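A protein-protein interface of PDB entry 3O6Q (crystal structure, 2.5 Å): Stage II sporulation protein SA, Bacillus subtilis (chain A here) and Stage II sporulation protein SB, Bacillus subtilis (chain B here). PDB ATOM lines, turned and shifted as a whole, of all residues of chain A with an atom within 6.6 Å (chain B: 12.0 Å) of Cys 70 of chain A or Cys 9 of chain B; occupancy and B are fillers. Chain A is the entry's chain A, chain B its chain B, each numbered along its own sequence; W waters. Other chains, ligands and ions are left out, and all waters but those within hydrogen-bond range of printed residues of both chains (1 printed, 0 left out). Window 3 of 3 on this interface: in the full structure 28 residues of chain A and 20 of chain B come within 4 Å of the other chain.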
ATOM      1  N   ASP A  53      -6.151  -6.524 -12.218  1.00  0.00           N
ATOM      2  CA  ASP A  53      -7.056  -6.176 -13.325  1.00  0.00           C
ATOM      3  C   ASP A  53      -7.585  -7.411 -14.113  1.00  0.00           C
ATOM      4  O   ASP A  53      -8.773  -7.465 -14.388  1.00  0.00           O
ATOM      5  CB  ASP A  53      -6.407  -5.184 -14.287  1.00  0.00           C
ATOM      6  CG  ASP A  53      -7.406  -4.558 -15.255  1.00  0.00           C
ATOM      7  OD1 ASP A  53      -8.387  -3.945 -14.788  1.00  0.00           O
ATOM      8  OD2 ASP A  53      -7.225  -4.679 -16.496  1.00  0.00           O
ATOM      9  N   LYS A  57     -11.511  -8.779 -14.104  1.00  0.00           N
ATOM     10  CA  LYS A  57     -12.177  -8.934 -15.384  1.00  0.00           C
ATOM     11  C   LYS A  57     -12.694 -10.331 -15.659  1.00  0.00           C
ATOM     12  O   LYS A  57     -13.770 -10.479 -16.213  1.00  0.00           O
ATOM     13  CB  LYS A  57     -11.279  -8.479 -16.516  1.00  0.00           C
ATOM     14  CG  LYS A  57     -11.352  -6.974 -16.702  1.00  0.00           C
ATOM     15  CD  LYS A  57     -10.266  -6.411 -17.563  1.00  0.00           C
ATOM     16  CE  LYS A  57     -10.394  -4.900 -17.578  1.00  0.00           C
ATOM     17  NZ  LYS A  57      -9.221  -4.305 -18.240  1.00  0.00           N
ATOM     18  N   ALA A  67     -15.649  -4.463 -14.420  1.00  0.00           N
ATOM     19  CA  ALA A  67     -14.651  -4.110 -13.413  1.00  0.00           C
ATOM     20  C   ALA A  67     -13.354  -3.685 -14.113  1.00  0.00           C
ATOM     21  O   ALA A  67     -13.003  -4.214 -15.177  1.00  0.00           O
ATOM     22  CB  ALA A  67     -14.409  -5.252 -12.481  1.00  0.00           C
ATOM     23  N   SER A  68     -12.665  -2.716 -13.511  1.00  0.00           N
ATOM     24  CA  SER A  68     -11.404  -2.186 -14.022  1.00  0.00           C
ATOM     25  C   SER A  68     -10.560  -1.733 -12.847  1.00  0.00           C
ATOM     26  O   SER A  68     -11.082  -1.459 -11.775  1.00  0.00           O
ATOM     27  CB  SER A  68     -11.625  -0.985 -14.914  1.00  0.00           C
ATOM     28  OG  SER A  68     -12.544  -1.251 -15.939  1.00  0.00           O
ATOM     29  N   LEU A  69      -9.258  -1.660 -13.085  1.00  0.00           N
ATOM     30  CA  LEU A  69      -8.292  -1.147 -12.148  1.00  0.00           C
ATOM     31  C   LEU A  69      -7.737   0.113 -12.774  1.00  0.00           C
ATOM     32  O   LEU A  69      -7.132   0.062 -13.838  1.00  0.00           O
ATOM     33  CB  LEU A  69      -7.176  -2.162 -11.924  1.00  0.00           C
ATOM     34  CG  LEU A  69      -6.242  -1.782 -10.752  1.00  0.00           C
ATOM     35  CD1 LEU A  69      -7.032  -1.512  -9.492  1.00  0.00           C
ATOM     36  CD2 LEU A  69      -5.223  -2.847 -10.441  1.00  0.00           C
ATOM     37  N   CYS A  70      -7.978   1.255 -12.136  1.00  0.00           N
ATOM     38  CA  CYS A  70      -7.661   2.530 -12.735  1.00  0.00           C
ATOM     39  C   CYS A  70      -6.566   3.209 -11.930  1.00  0.00           C
ATOM     40  O   CYS A  70      -6.604   3.210 -10.702  1.00  0.00           O
ATOM     41  CB  CYS A  70      -8.920   3.406 -12.798  1.00  0.00           C
ATOM     42  SG  CYS A  70     -10.224   2.778 -13.853  1.00  0.00           S
ATOM     43  N   HIS A  71      -5.580   3.769 -12.627  1.00  0.00           N
ATOM     44  CA  HIS A  71      -4.553   4.548 -11.966  1.00  0.00           C
ATOM     45  C   HIS A  71      -5.253   5.701 -11.271  1.00  0.00           C
ATOM     46  O   HIS A  71      -6.247   6.220 -11.776  1.00  0.00           O
ATOM     47  CB  HIS A  71      -3.514   5.057 -12.974  1.00  0.00           C
ATOM     48  CG  HIS A  71      -2.574   3.993 -13.470  1.00  0.00           C
ATOM     49  ND1 HIS A  71      -1.446   3.610 -12.771  1.00  0.00           N
ATOM     50  CD2 HIS A  71      -2.601   3.226 -14.593  1.00  0.00           C
ATOM     51  CE1 HIS A  71      -0.823   2.651 -13.440  1.00  0.00           C
ATOM     52  NE2 HIS A  71      -1.507   2.395 -14.544  1.00  0.00           N
ATOM     53  N   TYR A  72      -4.768   6.066 -10.097  1.00  0.00           N
ATOM     54  CA  TYR A  72      -5.323   7.185  -9.366  1.00  0.00           C
ATOM     55  C   TYR A  72      -4.184   7.956  -8.683  1.00  0.00           C
ATOM     56  O   TYR A  72      -4.232   8.248  -7.487  1.00  0.00           O
ATOM     57  CB  TYR A  72      -6.386   6.692  -8.377  1.00  0.00           C
ATOM     58  CG  TYR A  72      -7.250   7.818  -7.845  1.00  0.00           C
ATOM     59  CD1 TYR A  72      -8.315   8.319  -8.583  1.00  0.00           C
ATOM     60  CD2 TYR A  72      -6.989   8.394  -6.619  1.00  0.00           C
ATOM     61  CE1 TYR A  72      -9.084   9.376  -8.117  1.00  0.00           C
ATOM     62  CE2 TYR A  72      -7.759   9.438  -6.143  1.00  0.00           C
ATOM     63  CZ  TYR A  72      -8.806   9.931  -6.893  1.00  0.00           C
ATOM     64  OH  TYR A  72      -9.553  10.997  -6.411  1.00  0.00           O
ATOM     65  N   SER A  73      -3.171   8.279  -9.493  1.00  0.00           N
ATOM     66  CA  SER A  73      -1.969   8.975  -9.059  1.00  0.00           C
ATOM     67  C   SER A  73      -1.939  10.432  -9.507  1.00  0.00           C
ATOM     68  O   SER A  73      -1.859  11.350  -8.699  1.00  0.00           O
ATOM     69  CB  SER A  73      -0.740   8.283  -9.656  1.00  0.00           C
ATOM     70  OG  SER A  73      -0.687   6.962  -9.231  1.00  0.00           O
ATOM     71  N   ASP A  77      -5.255  11.209 -14.108  1.00  0.00           N
ATOM     72  CA  ASP A  77      -5.930   9.969 -13.720  1.00  0.00           C
ATOM     73  C   ASP A  77      -7.215  10.246 -12.972  1.00  0.00           C
ATOM     74  O   ASP A  77      -8.235   9.577 -13.180  1.00  0.00           O
ATOM     75  CB  ASP A  77      -5.033   9.103 -12.817  1.00  0.00           C
ATOM     76  CG  ASP A  77      -3.739   8.695 -13.489  1.00  0.00           C
ATOM     77  OD1 ASP A  77      -3.725   8.637 -14.729  1.00  0.00           O
ATOM     78  OD2 ASP A  77      -2.742   8.461 -12.765  1.00  0.00           O
ATOM     79  N   LEU A  81     -11.292   9.774 -14.244  1.00  0.00           N
ATOM     80  CA  LEU A  81     -12.257   8.999 -13.482  1.00  0.00           C
ATOM     81  C   LEU A  81     -13.525   9.823 -13.200  1.00  0.00           C
ATOM     82  O   LEU A  81     -14.618   9.387 -13.541  1.00  0.00           O
ATOM     83  CB  LEU A  81     -11.598   8.504 -12.194  1.00  0.00           C
ATOM     84  CG  LEU A  81     -12.071   7.185 -11.619  1.00  0.00           C
ATOM     85  CD1 LEU A  81     -12.099   6.111 -12.660  1.00  0.00           C
ATOM     86  CD2 LEU A  81     -11.095   6.797 -10.547  1.00  0.00           C
ATOM     87  N   PHE A 113      -7.774   1.795  -3.924  1.00  0.00           N
ATOM     88  CA  PHE A 113      -6.972   0.616  -3.751  1.00  0.00           C
ATOM     89  C   PHE A 113      -5.502   0.979  -3.919  1.00  0.00           C
ATOM     90  O   PHE A 113      -5.142   1.778  -4.788  1.00  0.00           O
ATOM     91  CB  PHE A 113      -7.431  -0.406  -4.794  1.00  0.00           C
ATOM     92  CG  PHE A 113      -6.676  -1.674  -4.764  1.00  0.00           C
ATOM     93  CD1 PHE A 113      -6.781  -2.510  -3.691  1.00  0.00           C
ATOM     94  CD2 PHE A 113      -5.874  -2.037  -5.824  1.00  0.00           C
ATOM     95  CE1 PHE A 113      -6.123  -3.708  -3.666  1.00  0.00           C
ATOM     96  CE2 PHE A 113      -5.180  -3.235  -5.817  1.00  0.00           C
ATOM     97  CZ  PHE A 113      -5.305  -4.078  -4.731  1.00  0.00           C
ATOM     98  N   ASN A 119      -1.337   4.309  -6.021  1.00  0.00           N
ATOM     99  CA  ASN A 119      -2.778   4.454  -5.842  1.00  0.00           C
ATOM    100  C   ASN A 119      -3.554   4.105  -7.079  1.00  0.00           C
ATOM    101  O   ASN A 119      -3.204   4.486  -8.183  1.00  0.00           O
ATOM    102  CB  ASN A 119      -3.130   5.873  -5.403  1.00  0.00           C
ATOM    103  CG  ASN A 119      -2.622   6.179  -3.983  1.00  0.00           C
ATOM    104  OD1 ASN A 119      -2.382   5.279  -3.188  1.00  0.00           O
ATOM    105  ND2 ASN A 119      -2.418   7.443  -3.693  1.00  0.00           N
ATOM    106  N   TYR A 120      -4.637   3.384  -6.857  1.00  0.00           N
ATOM    107  CA  TYR A 120      -5.538   2.989  -7.898  1.00  0.00           C
ATOM    108  C   TYR A 120      -6.966   3.104  -7.376  1.00  0.00           C
ATOM    109  O   TYR A 120      -7.191   3.410  -6.191  1.00  0.00           O
ATOM    110  CB  TYR A 120      -5.284   1.520  -8.309  1.00  0.00           C
ATOM    111  CG  TYR A 120      -3.921   1.221  -8.891  1.00  0.00           C
ATOM    112  CD1 TYR A 120      -3.746   1.181 -10.259  1.00  0.00           C
ATOM    113  CD2 TYR A 120      -2.823   0.953  -8.079  1.00  0.00           C
ATOM    114  CE1 TYR A 120      -2.519   0.900 -10.819  1.00  0.00           C
ATOM    115  CE2 TYR A 120      -1.563   0.662  -8.637  1.00  0.00           C
ATOM    116  CZ  TYR A 120      -1.426   0.638 -10.021  1.00  0.00           C
ATOM    117  OH  TYR A 120      -0.222   0.357 -10.649  1.00  0.00           O
ATOM    118  N   VAL A 121      -7.923   2.875  -8.276  1.00  0.00           N
ATOM    119  CA  VAL A 121      -9.316   2.799  -7.908  1.00  0.00           C
ATOM    120  C   VAL A 121      -9.902   1.644  -8.686  1.00  0.00           C
ATOM    121  O   VAL A 121      -9.749   1.575  -9.877  1.00  0.00           O
ATOM    122  CB  VAL A 121     -10.048   4.140  -8.190  1.00  0.00           C
ATOM    123  CG1 VAL A 121     -11.534   3.992  -8.039  1.00  0.00           C
ATOM    124  CG2 VAL A 121      -9.561   5.198  -7.245  1.00  0.00           C
ATOM    125  N   ILE A 122     -10.484   0.687  -7.989  1.00  0.00           N
ATOM    126  CA  ILE A 122     -11.220  -0.369  -8.632  1.00  0.00           C
ATOM    127  C   ILE A 122     -12.591   0.206  -9.014  1.00  0.00           C
ATOM    128  O   ILE A 122     -13.399   0.513  -8.141  1.00  0.00           O
ATOM    129  CB  ILE A 122     -11.408  -1.582  -7.691  1.00  0.00           C
ATOM    130  CG1 ILE A 122     -10.076  -2.197  -7.272  1.00  0.00           C
ATOM    131  CG2 ILE A 122     -12.224  -2.687  -8.393  1.00  0.00           C
ATOM    132  CD1 ILE A 122     -10.182  -2.947  -5.928  1.00  0.00           C
ATOM    133  N   LYS A 123     -12.839   0.344 -10.312  1.00  0.00           N
ATOM    134  CA  LYS A 123     -14.123   0.780 -10.834  1.00  0.00           C
ATOM    135  C   LYS A 123     -15.041  -0.378 -11.144  1.00  0.00           C
ATOM    136  O   LYS A 123     -14.731  -1.174 -12.016  1.00  0.00           O
ATOM    137  CB  LYS A 123     -13.903   1.564 -12.118  1.00  0.00           C
ATOM    138  CG  LYS A 123     -15.156   2.184 -12.747  1.00  0.00           C
ATOM    139  CD  LYS A 123     -14.772   3.101 -13.892  1.00  0.00           C
ATOM    140  CE  LYS A 123     -15.990   3.633 -14.640  1.00  0.00           C
ATOM    141  NZ  LYS A 123     -15.650   4.391 -15.908  1.00  0.00           N
ATOM    142  N   CYS B   9      -9.036   2.246 -18.979  1.00  0.00           N
ATOM    143  CA  CYS B   9      -8.514   1.678 -17.675  1.00  0.00           C
ATOM    144  C   CYS B   9      -8.047   0.233 -17.767  1.00  0.00           C
ATOM    145  O   CYS B   9      -8.831  -0.691 -17.560  1.00  0.00           O
ATOM    146  CB  CYS B   9      -9.578   1.766 -16.581  1.00  0.00           C
ATOM    147  SG  CYS B   9      -9.660   3.325 -15.742  1.00  0.00           S
ATOM    148  N   GLU B  10      -6.762   0.032 -18.024  1.00  0.00           N
ATOM    149  CA  GLU B  10      -6.292  -1.293 -18.356  1.00  0.00           C
ATOM    150  C   GLU B  10      -4.770  -1.364 -18.133  1.00  0.00           C
ATOM    151  O   GLU B  10      -3.999  -1.318 -19.089  1.00  0.00           O
ATOM    152  CB  GLU B  10      -6.678  -1.572 -19.812  1.00  0.00           C
ATOM    153  CG  GLU B  10      -6.483  -2.995 -20.276  1.00  0.00           C
ATOM    154  CD  GLU B  10      -6.530  -3.099 -21.779  1.00  0.00           C
ATOM    155  OE1 GLU B  10      -6.908  -2.101 -22.427  1.00  0.00           O
ATOM    156  OE2 GLU B  10      -6.206  -4.180 -22.311  1.00  0.00           O
ATOM    157  N   PRO B  11      -4.337  -1.454 -16.858  1.00  0.00           N
ATOM    158  CA  PRO B  11      -2.915  -1.463 -16.534  1.00  0.00           C
ATOM    159  C   PRO B  11      -2.245  -2.749 -17.010  1.00  0.00           C
ATOM    160  O   PRO B  11      -2.739  -3.837 -16.721  1.00  0.00           O
ATOM    161  CB  PRO B  11      -2.883  -1.337 -14.997  1.00  0.00           C
ATOM    162  CG  PRO B  11      -4.191  -1.739 -14.536  1.00  0.00           C
ATOM    163  CD  PRO B  11      -5.178  -1.496 -15.647  1.00  0.00           C
ATOM    164  N   ARG B  12      -1.173  -2.605 -17.785  1.00  0.00           N
ATOM    165  CA  ARG B  12      -0.411  -3.734 -18.300  1.00  0.00           C
ATOM    166  C   ARG B  12       1.074  -3.539 -17.984  1.00  0.00           C
ATOM    167  O   ARG B  12       1.525  -2.399 -17.887  1.00  0.00           O
ATOM    168  CB  ARG B  12      -0.648  -3.880 -19.817  1.00  0.00           C
ATOM    169  CG  ARG B  12      -2.111  -4.218 -20.194  1.00  0.00           C
ATOM    170  CD  ARG B  12      -2.518  -5.662 -19.797  1.00  0.00           C
ATOM    171  NE  ARG B  12      -3.958  -5.941 -19.936  1.00  0.00           N
ATOM    172  CZ  ARG B  12      -4.887  -5.739 -18.988  1.00  0.00           C
ATOM    173  NH1 ARG B  12      -4.564  -5.226 -17.793  1.00  0.00           N
ATOM    174  NH2 ARG B  12      -6.165  -6.044 -19.239  1.00  0.00           N
ATOM    175  N   ALA B  13       1.811  -4.641 -17.808  1.00  0.00           N
ATOM    176  CA  ALA B  13       3.254  -4.596 -17.458  1.00  0.00           C
ATOM    177  C   ALA B  13       4.145  -4.956 -18.622  1.00  0.00           C
ATOM    178  O   ALA B  13       3.744  -5.686 -19.516  1.00  0.00           O
ATOM    179  CB  ALA B  13       3.566  -5.520 -16.300  1.00  0.00           C
HETATM  180  O   HOH W   1      -6.138   3.395 -15.860  1.00  0.00           O
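The guanidinium group of Arg 12 of chain B is in salt-bridge range of the side-chain carboxylate of Asp 53 of chain A.
The side-chain sulfur (SG) of Cys 70 of chain A forms a disulfide with the side-chain sulfur (SG) of Cys 9 of chain B (2.0 Å).
The backbone carbonyl oxygen (O) of Ser 68 of chain A lies within hydrogen-bond range of the backbone NH (N) of Lys 123 of chain A (2.9 Å).
The side-chain carboxylate (OE2) of Glu 10 of chain B is in salt-bridge range of the guanidinium group (NH2) of Arg 12 of chain B, at 3.6 Å.
The side-chain carboxylate (OD2) of Asp 53 of chain A lies within salt-bridge range of the side-chain amino group (NZ) of Lys 57 of chain A, 2.7 Å away.
N of Val 121 of chain A lies within hydrogen-bond range of O of Cys 70 of chain A, 2.8 Å away.
The side-chain carboxylate (OD1) of Asp 53 of chain A is in hydrogen-bond range of the backbone NH (N) of Leu 69 of chain A (3.0 Å).
Among the printed residues, pairs that only touch across the chains: Leu 69 of chain A with Pro 11 of chain B (3.1 Å), Lys 57 of chain A with Glu 10 of chain B (3.7 Å), Lys 57 of chain A with Arg 12 of chain B (3.7 Å), Lys 57 of chain A with Cys 9 of chain B (3.7 Å), Asp 53 of chain A with Pro 11 of chain B (3.8 Å), Ser 68 of chain A with Cys 9 of chain B (3.8 Å) and Asp 53 of chain A with Glu 10 of chain B (3.97 Å).
Of chain B, only Cys 9 (2.0 Å) comes within 4 Å of Cys 70 of chain A.
Of chain A, only Lys 57, Ser 68 and Cys 70 come within 4 Å of Cys 9 of chain B.
Leu 69 of chain A touches just one residue of chain B: Pro 11 (3.1 Å).
No residue of chain B comes within 4 Å of Leu 81 of chain A.
Tyr 120 of chain A touches none of the printed residues of chain B.
No residue of chain B comes within 4 Å of Val 121 of chain A.
No residue of chain B comes within 4 Å of Ile 122 of chain A.
Of the printed residues of chain A, Arg 12 of chain B touches Asp 53 (3.0 Å) and Lys 57 (3.7 Å).
Printed residues of chain B within 4 Å of Lys 57 of chain A: Cys 9 (3.7 Å), Glu 10 (3.7 Å) and Arg 12 (3.7 Å).
Of the printed residues of chain A, Pro 11 of chain B touches Asp 53 (3.8 Å) and Leu 69 (3.1 Å).
Of the printed residues of chain A, Glu 10 of chain B touches Asp 53 (3.97 Å) and Lys 57 (3.7 Å).
Tyr 72 of chain A touches none of the printed residues of chain B.
The nearest residue of chain A that does not touch Cys 9 of chain B is Leu 69 of chain A (4.04 Å).
Hydrophobic or aromatic side chains of chain A that line the printed part of chain B: Leu 69.
Of the 5 printed residues of chain B, 4 touch a printed residue of chain A.
Hydrophobic or aromatic side chains of chain B within 4 Å of the printed part of chain A: Pro 11.
Among the printed residues, 9 pairs touch across the chains.
Among the printed residues, Asp or Glu carboxylates within 4 Å of a Lys or Arg side-chain nitrogen of the other chain: Asp 53 of chain A with Arg 12 of chain B (3.0 Å).
Water W1 bridges N of His 71 of chain A (3.3 Å) and SG of Cys 9 of chain B (3.5 Å).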
